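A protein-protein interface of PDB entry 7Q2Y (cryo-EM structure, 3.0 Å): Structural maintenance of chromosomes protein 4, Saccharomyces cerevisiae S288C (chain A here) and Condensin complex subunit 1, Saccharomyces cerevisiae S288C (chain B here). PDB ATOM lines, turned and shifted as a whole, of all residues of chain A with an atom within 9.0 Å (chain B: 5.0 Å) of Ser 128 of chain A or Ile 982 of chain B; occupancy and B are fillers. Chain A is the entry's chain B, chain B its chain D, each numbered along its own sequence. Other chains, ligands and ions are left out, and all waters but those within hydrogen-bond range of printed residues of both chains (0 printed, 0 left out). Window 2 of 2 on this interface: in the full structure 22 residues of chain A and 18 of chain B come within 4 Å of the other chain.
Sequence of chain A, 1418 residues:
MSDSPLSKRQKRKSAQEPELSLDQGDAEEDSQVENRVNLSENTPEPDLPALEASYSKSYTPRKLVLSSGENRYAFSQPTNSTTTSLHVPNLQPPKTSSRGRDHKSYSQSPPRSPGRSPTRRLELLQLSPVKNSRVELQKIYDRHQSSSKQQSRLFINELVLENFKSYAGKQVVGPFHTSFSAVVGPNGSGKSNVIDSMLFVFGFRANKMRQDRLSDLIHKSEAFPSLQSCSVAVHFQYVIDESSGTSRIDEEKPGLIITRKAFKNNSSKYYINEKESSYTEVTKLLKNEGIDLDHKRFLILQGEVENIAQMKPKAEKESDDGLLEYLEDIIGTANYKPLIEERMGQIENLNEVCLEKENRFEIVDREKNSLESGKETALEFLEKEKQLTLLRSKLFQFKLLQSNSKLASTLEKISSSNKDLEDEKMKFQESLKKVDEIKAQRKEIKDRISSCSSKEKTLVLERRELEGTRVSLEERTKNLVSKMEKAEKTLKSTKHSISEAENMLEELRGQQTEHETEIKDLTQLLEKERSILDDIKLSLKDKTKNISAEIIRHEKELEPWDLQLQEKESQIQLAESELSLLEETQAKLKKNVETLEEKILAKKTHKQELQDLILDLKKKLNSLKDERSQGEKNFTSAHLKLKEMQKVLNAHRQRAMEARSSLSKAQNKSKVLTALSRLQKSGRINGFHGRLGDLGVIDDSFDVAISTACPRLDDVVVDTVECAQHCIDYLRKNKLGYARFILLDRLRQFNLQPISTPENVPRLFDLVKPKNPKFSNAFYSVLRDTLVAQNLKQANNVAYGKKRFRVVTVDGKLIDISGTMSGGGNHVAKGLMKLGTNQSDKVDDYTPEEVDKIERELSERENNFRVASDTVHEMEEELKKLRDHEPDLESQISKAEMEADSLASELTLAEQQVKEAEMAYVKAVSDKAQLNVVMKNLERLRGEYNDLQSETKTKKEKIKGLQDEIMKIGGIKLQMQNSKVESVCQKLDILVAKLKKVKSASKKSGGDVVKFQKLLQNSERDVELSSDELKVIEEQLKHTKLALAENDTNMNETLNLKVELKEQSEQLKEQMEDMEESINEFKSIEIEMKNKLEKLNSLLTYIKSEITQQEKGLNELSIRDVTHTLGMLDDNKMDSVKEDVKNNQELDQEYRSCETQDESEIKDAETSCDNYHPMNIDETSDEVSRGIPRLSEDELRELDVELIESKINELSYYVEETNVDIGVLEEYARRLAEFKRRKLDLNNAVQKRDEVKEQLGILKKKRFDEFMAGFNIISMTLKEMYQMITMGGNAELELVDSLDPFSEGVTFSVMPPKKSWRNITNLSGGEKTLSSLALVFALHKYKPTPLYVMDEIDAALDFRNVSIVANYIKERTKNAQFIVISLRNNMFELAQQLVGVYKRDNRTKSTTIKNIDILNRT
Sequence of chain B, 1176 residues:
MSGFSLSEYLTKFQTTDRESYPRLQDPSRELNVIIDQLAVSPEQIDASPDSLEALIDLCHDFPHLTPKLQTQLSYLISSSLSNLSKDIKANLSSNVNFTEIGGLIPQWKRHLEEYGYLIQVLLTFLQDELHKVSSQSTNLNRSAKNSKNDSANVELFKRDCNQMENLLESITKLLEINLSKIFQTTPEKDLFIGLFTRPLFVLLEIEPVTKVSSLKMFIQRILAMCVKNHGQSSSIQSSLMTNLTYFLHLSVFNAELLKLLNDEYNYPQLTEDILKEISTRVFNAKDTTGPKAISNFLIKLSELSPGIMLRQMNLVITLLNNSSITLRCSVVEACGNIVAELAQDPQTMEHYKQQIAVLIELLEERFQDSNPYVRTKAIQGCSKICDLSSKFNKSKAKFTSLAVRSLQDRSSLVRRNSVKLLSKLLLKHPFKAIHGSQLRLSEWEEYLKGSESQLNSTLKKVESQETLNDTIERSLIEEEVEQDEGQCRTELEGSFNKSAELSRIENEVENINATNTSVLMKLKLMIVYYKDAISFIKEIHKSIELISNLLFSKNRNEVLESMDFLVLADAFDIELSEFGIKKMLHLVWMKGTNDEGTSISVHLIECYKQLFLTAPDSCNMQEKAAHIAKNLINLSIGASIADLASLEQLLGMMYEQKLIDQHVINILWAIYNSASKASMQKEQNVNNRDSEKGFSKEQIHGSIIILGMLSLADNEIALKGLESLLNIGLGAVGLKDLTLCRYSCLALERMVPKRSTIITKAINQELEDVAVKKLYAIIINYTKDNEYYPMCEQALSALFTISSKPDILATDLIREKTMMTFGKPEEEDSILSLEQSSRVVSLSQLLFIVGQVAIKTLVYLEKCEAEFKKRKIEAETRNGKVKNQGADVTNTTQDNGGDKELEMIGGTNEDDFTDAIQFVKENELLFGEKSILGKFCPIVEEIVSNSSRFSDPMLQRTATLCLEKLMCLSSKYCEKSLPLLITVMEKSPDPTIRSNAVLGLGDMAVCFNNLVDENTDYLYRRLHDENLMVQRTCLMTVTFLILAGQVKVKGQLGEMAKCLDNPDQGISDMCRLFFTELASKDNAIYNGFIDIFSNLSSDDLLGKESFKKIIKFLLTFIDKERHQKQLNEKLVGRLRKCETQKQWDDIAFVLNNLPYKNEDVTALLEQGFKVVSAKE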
ATOM      1  N   GLN A 126      27.396 -12.745   2.050  1.00  0.00           N
ATOM      2  CA  GLN A 126      27.090 -13.882   2.908  1.00  0.00           C
ATOM      3  C   GLN A 126      27.751 -13.723   4.275  1.00  0.00           C
ATOM      4  O   GLN A 126      27.305 -14.306   5.263  1.00  0.00           O
ATOM      5  CB  GLN A 126      27.541 -15.189   2.248  1.00  0.00           C
ATOM      6  CG  GLN A 126      26.987 -16.444   2.904  1.00  0.00           C
ATOM      7  CD  GLN A 126      27.373 -17.709   2.163  1.00  0.00           C
ATOM      8  OE1 GLN A 126      28.108 -17.663   1.175  1.00  0.00           O
ATOM      9  NE2 GLN A 126      26.880 -18.847   2.636  1.00  0.00           N
ATOM     10  N   LEU A 127      28.813 -12.926   4.324  1.00  0.00           N
ATOM     11  CA  LEU A 127      29.556 -12.683   5.553  1.00  0.00           C
ATOM     12  C   LEU A 127      29.184 -11.317   6.115  1.00  0.00           C
ATOM     13  O   LEU A 127      29.288 -10.302   5.419  1.00  0.00           O
ATOM     14  CB  LEU A 127      31.063 -12.760   5.305  1.00  0.00           C
ATOM     15  CG  LEU A 127      31.616 -14.141   4.948  1.00  0.00           C
ATOM     16  CD1 LEU A 127      33.089 -14.053   4.577  1.00  0.00           C
ATOM     17  CD2 LEU A 127      31.407 -15.114   6.098  1.00  0.00           C
ATOM     18  N   SER A 128      28.749 -11.300   7.373  1.00  0.00           N
ATOM     19  CA  SER A 128      28.375 -10.054   8.018  1.00  0.00           C
ATOM     20  C   SER A 128      29.611  -9.188   8.261  1.00  0.00           C
ATOM     21  O   SER A 128      30.697  -9.704   8.536  1.00  0.00           O
ATOM     22  CB  SER A 128      27.665 -10.330   9.340  1.00  0.00           C
ATOM     23  OG  SER A 128      28.327 -11.349  10.068  1.00  0.00           O
ATOM     24  N   PRO A 129      29.471  -7.868   8.157  1.00  0.00           N
ATOM     25  CA  PRO A 129      30.623  -6.988   8.388  1.00  0.00           C
ATOM     26  C   PRO A 129      31.086  -7.031   9.835  1.00  0.00           C
ATOM     27  O   PRO A 129      30.297  -7.225  10.763  1.00  0.00           O
ATOM     28  CB  PRO A 129      30.089  -5.599   8.017  1.00  0.00           C
ATOM     29  CG  PRO A 129      28.612  -5.704   8.200  1.00  0.00           C
ATOM     30  CD  PRO A 129      28.251  -7.112   7.827  1.00  0.00           C
ATOM     31  N   VAL A 130      32.391  -6.847  10.017  1.00  0.00           N
ATOM     32  CA  VAL A 130      33.016  -6.828  11.333  1.00  0.00           C
ATOM     33  C   VAL A 130      33.940  -5.622  11.412  1.00  0.00           C
ATOM     34  O   VAL A 130      34.580  -5.249  10.422  1.00  0.00           O
ATOM     35  CB  VAL A 130      33.793  -8.130  11.622  1.00  0.00           C
ATOM     36  CG1 VAL A 130      32.834  -9.299  11.780  1.00  0.00           C
ATOM     37  CG2 VAL A 130      34.801  -8.406  10.517  1.00  0.00           C
ATOM     38  N   LYS A 131      33.999  -5.003  12.588  1.00  0.00           N
ATOM     39  CA  LYS A 131      34.863  -3.847  12.820  1.00  0.00           C
ATOM     40  C   LYS A 131      36.198  -4.352  13.353  1.00  0.00           C
ATOM     41  O   LYS A 131      36.370  -4.536  14.559  1.00  0.00           O
ATOM     42  CB  LYS A 131      34.206  -2.867  13.784  1.00  0.00           C
ATOM     43  CG  LYS A 131      32.961  -2.194  13.231  1.00  0.00           C
ATOM     44  CD  LYS A 131      32.455  -1.111  14.169  1.00  0.00           C
ATOM     45  CE  LYS A 131      31.787  -1.710  15.395  1.00  0.00           C
ATOM     46  NZ  LYS A 131      31.187  -0.663  16.267  1.00  0.00           N
ATOM     47  N   LEU B 978      36.538 -14.883  12.925  1.00  0.00           N
ATOM     48  CA  LEU B 978      35.427 -14.271  13.653  1.00  0.00           C
ATOM     49  C   LEU B 978      34.209 -13.979  12.782  1.00  0.00           C
ATOM     50  O   LEU B 978      33.081 -14.222  13.246  1.00  0.00           O
ATOM     51  CB  LEU B 978      35.923 -13.007  14.362  1.00  0.00           C
ATOM     52  CG  LEU B 978      34.919 -12.279  15.257  1.00  0.00           C
ATOM     53  CD1 LEU B 978      34.406 -13.204  16.348  1.00  0.00           C
ATOM     54  CD2 LEU B 978      35.550 -11.035  15.861  1.00  0.00           C
ATOM     55  N   PRO B 979      34.336 -13.421  11.568  1.00  0.00           N
ATOM     56  CA  PRO B 979      33.126 -13.222  10.749  1.00  0.00           C
ATOM     57  C   PRO B 979      32.383 -14.512  10.455  1.00  0.00           C
ATOM     58  O   PRO B 979      31.146 -14.521  10.434  1.00  0.00           O
ATOM     59  CB  PRO B 979      33.671 -12.574   9.468  1.00  0.00           C
ATOM     60  CG  PRO B 979      34.954 -11.954   9.875  1.00  0.00           C
ATOM     61  CD  PRO B 979      35.531 -12.870  10.903  1.00  0.00           C
ATOM     62  N   LEU B 980      33.109 -15.609  10.237  1.00  0.00           N
ATOM     63  CA  LEU B 980      32.457 -16.890   9.987  1.00  0.00           C
ATOM     64  C   LEU B 980      31.655 -17.345  11.200  1.00  0.00           C
ATOM     65  O   LEU B 980      30.513 -17.801  11.064  1.00  0.00           O
ATOM     66  CB  LEU B 980      33.503 -17.935   9.601  1.00  0.00           C
ATOM     67  CG  LEU B 980      33.016 -19.331   9.217  1.00  0.00           C
ATOM     68  CD1 LEU B 980      32.045 -19.262   8.052  1.00  0.00           C
ATOM     69  CD2 LEU B 980      34.209 -20.202   8.868  1.00  0.00           C
ATOM     70  N   LEU B 981      32.230 -17.212  12.398  1.00  0.00           N
ATOM     71  CA  LEU B 981      31.506 -17.576  13.611  1.00  0.00           C
ATOM     72  C   LEU B 981      30.295 -16.677  13.823  1.00  0.00           C
ATOM     73  O   LEU B 981      29.237 -17.144  14.259  1.00  0.00           O
ATOM     74  CB  LEU B 981      32.437 -17.513  14.820  1.00  0.00           C
ATOM     75  CG  LEU B 981      31.795 -17.942  16.140  1.00  0.00           C
ATOM     76  CD1 LEU B 981      31.455 -19.421  16.101  1.00  0.00           C
ATOM     77  CD2 LEU B 981      32.704 -17.626  17.318  1.00  0.00           C
ATOM     78  N   ILE B 982      30.432 -15.382  13.526  1.00  0.00           N
ATOM     79  CA  ILE B 982      29.308 -14.463  13.677  1.00  0.00           C
ATOM     80  C   ILE B 982      28.174 -14.853  12.737  1.00  0.00           C
ATOM     81  O   ILE B 982      27.001 -14.888  13.131  1.00  0.00           O
ATOM     82  CB  ILE B 982      29.770 -13.013  13.441  1.00  0.00           C
ATOM     83  CG1 ILE B 982      30.612 -12.524  14.621  1.00  0.00           C
ATOM     84  CG2 ILE B 982      28.576 -12.096  13.233  1.00  0.00           C
ATOM     85  CD1 ILE B 982      29.854 -12.453  15.923  1.00  0.00           C
ATOM     86  N   THR B 983      28.507 -15.162  11.480  1.00  0.00           N
ATOM     87  CA  THR B 983      27.490 -15.587  10.523  1.00  0.00           C
ATOM     88  C   THR B 983      26.838 -16.896  10.951  1.00  0.00           C
ATOM     89  O   THR B 983      25.623 -17.071  10.797  1.00  0.00           O
ATOM     90  CB  THR B 983      28.097 -15.729   9.128  1.00  0.00           C
ATOM     91  OG1 THR B 983      29.214 -16.627   9.177  1.00  0.00           O
ATOM     92  CG2 THR B 983      28.550 -14.379   8.606  1.00  0.00           C
ATOM     93  N   VAL B 984      27.632 -17.835  11.472  1.00  0.00           N
ATOM     94  CA  VAL B 984      27.075 -19.098  11.949  1.00  0.00           C
ATOM     95  C   VAL B 984      26.093 -18.844  13.085  1.00  0.00           C
ATOM     96  O   VAL B 984      24.970 -19.359  13.085  1.00  0.00           O
ATOM     97  CB  VAL B 984      28.202 -20.055  12.375  1.00  0.00           C
ATOM     98  CG1 VAL B 984      27.661 -21.146  13.283  1.00  0.00           C
ATOM     99  CG2 VAL B 984      28.872 -20.661  11.152  1.00  0.00           C
ATOM    100  N   MET B 985      26.488 -18.014  14.051  1.00  0.00           N
ATOM    101  CA  MET B 985      25.599 -17.700  15.166  1.00  0.00           C
ATOM    102  C   MET B 985      24.319 -17.034  14.678  1.00  0.00           C
ATOM    103  O   MET B 985      23.229 -17.313  15.190  1.00  0.00           O
ATOM    104  CB  MET B 985      26.311 -16.800  16.173  1.00  0.00           C
ATOM    105  CG  MET B 985      25.471 -16.469  17.397  1.00  0.00           C
ATOM    106  SD  MET B 985      26.336 -15.423  18.580  1.00  0.00           S
ATOM    107  CE  MET B 985      26.343 -13.867  17.694  1.00  0.00           C
ATOM    108  N   GLU B 986      24.433 -16.153  13.684  1.00  0.00           N
ATOM    109  CA  GLU B 986      23.267 -15.418  13.208  1.00  0.00           C
ATOM    110  C   GLU B 986      22.309 -16.301  12.415  1.00  0.00           C
ATOM    111  O   GLU B 986      21.088 -16.146  12.531  1.00  0.00           O
ATOM    112  CB  GLU B 986      23.712 -14.227  12.360  1.00  0.00           C
ATOM    113  CG  GLU B 986      23.881 -12.935  13.143  1.00  0.00           C
ATOM    114  CD  GLU B 986      23.922 -11.711  12.250  1.00  0.00           C
ATOM    115  OE1 GLU B 986      23.420 -11.788  11.110  1.00  0.00           O
ATOM    116  OE2 GLU B 986      24.458 -10.672  12.690  1.00  0.00           O
ATOM    117  N   LEU B1001      31.842 -16.833  21.955  1.00  0.00           N
ATOM    118  CA  LEU B1001      31.981 -15.380  21.953  1.00  0.00           C
ATOM    119  C   LEU B1001      32.246 -14.846  23.355  1.00  0.00           C
ATOM    120  O   LEU B1001      33.019 -13.902  23.528  1.00  0.00           O
ATOM    121  CB  LEU B1001      30.739 -14.728  21.352  1.00  0.00           C
ATOM    122  CG  LEU B1001      30.803 -14.511  19.839  1.00  0.00           C
ATOM    123  CD1 LEU B1001      29.543 -13.829  19.348  1.00  0.00           C
ATOM    124  CD2 LEU B1001      32.031 -13.699  19.463  1.00  0.00           C
ATOM    125  N   TYR B1018      27.112  -8.072  18.612  1.00  0.00           N
ATOM    126  CA  TYR B1018      26.444  -9.302  18.195  1.00  0.00           C
ATOM    127  C   TYR B1018      26.026 -10.141  19.397  1.00  0.00           C
ATOM    128  O   TYR B1018      24.906 -10.661  19.444  1.00  0.00           O
ATOM    129  CB  TYR B1018      27.348 -10.116  17.269  1.00  0.00           C
ATOM    130  CG  TYR B1018      27.665  -9.443  15.953  1.00  0.00           C
ATOM    131  CD1 TYR B1018      26.742  -9.439  14.915  1.00  0.00           C
ATOM    132  CD2 TYR B1018      28.894  -8.835  15.739  1.00  0.00           C
ATOM    133  CE1 TYR B1018      27.028  -8.830  13.708  1.00  0.00           C
ATOM    134  CE2 TYR B1018      29.189  -8.224  14.535  1.00  0.00           C
ATOM    135  CZ  TYR B1018      28.252  -8.226  13.524  1.00  0.00           C
ATOM    136  OH  TYR B1018      28.543  -7.621  12.323  1.00  0.00           O
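Among the printed residues, pairs that only touch across the chains: Ser 128 of chain A with Ile 982 of chain B (3.3 Å), Ser 128 of chain A with Thr 983 of chain B (3.3 Å), Gln 126 of chain A with Thr 983 of chain B (3.6 Å), Val 130 of chain A with Pro 979 of chain B (3.6 Å) and Leu 127 of chain A with Thr 983 of chain B (3.6 Å).
O of Pro 979 of chain B lies within hydrogen-bond range of OG1 of Thr 983 of chain B (3.1 Å).
O of Leu 980 of chain B lies within hydrogen-bond range of OG1 of Thr 983 of chain B (2.6 Å).
Printed residues of chain B that touch a printed residue of chain A: Pro 979, Ile 982, Thr 983 and Tyr 1018.
Hydrophobic or aromatic side chains of chain B within 4 Å of the printed part of chain A: Pro 979, Ile 982 and Tyr 1018.
Of the 6 printed residues of chain A, 5 touch a printed residue of chain B.
Among the printed residues, 6 pairs touch across the chains.
Among the printed residues, no Asp or Glu carboxylate lies within 4 Å of a Lys or Arg side-chain nitrogen of the other chain.
Ser 128 of chain A touches just these residues of chain B: Ile 982 (3.3 Å) and Thr 983 (3.3 Å).
Printed residues of chain A within 4 Å of Thr 983 of chain B: Gln 126 (3.6 Å), Leu 127 (3.6 Å) and Ser 128 (3.3 Å).
Of the printed residues of chain B, Val 130 of chain A touches Pro 979 (3.6 Å).
Of the printed residues of chain A, Tyr 1018 of chain B touches Pro 129 (2.4 Å).
Of the printed residues of chain B, Pro 129 of chain A touches Tyr 1018.
Of the printed residues of chain B, Leu 127 of chain A touches Thr 983.
Printed residues of chain A within 4 Å of Pro 979 of chain B: Val 130 (3.6 Å).
The nearest printed residue of chain B that does not touch Leu 127 of chain A is Pro 979 of chain B (4.4 Å).
The backbone carbonyl oxygen (O) of Pro 129 of chain A sits close to the side-chain hydroxyl (OH) of Tyr 1018 of chain B (2.4 Å).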
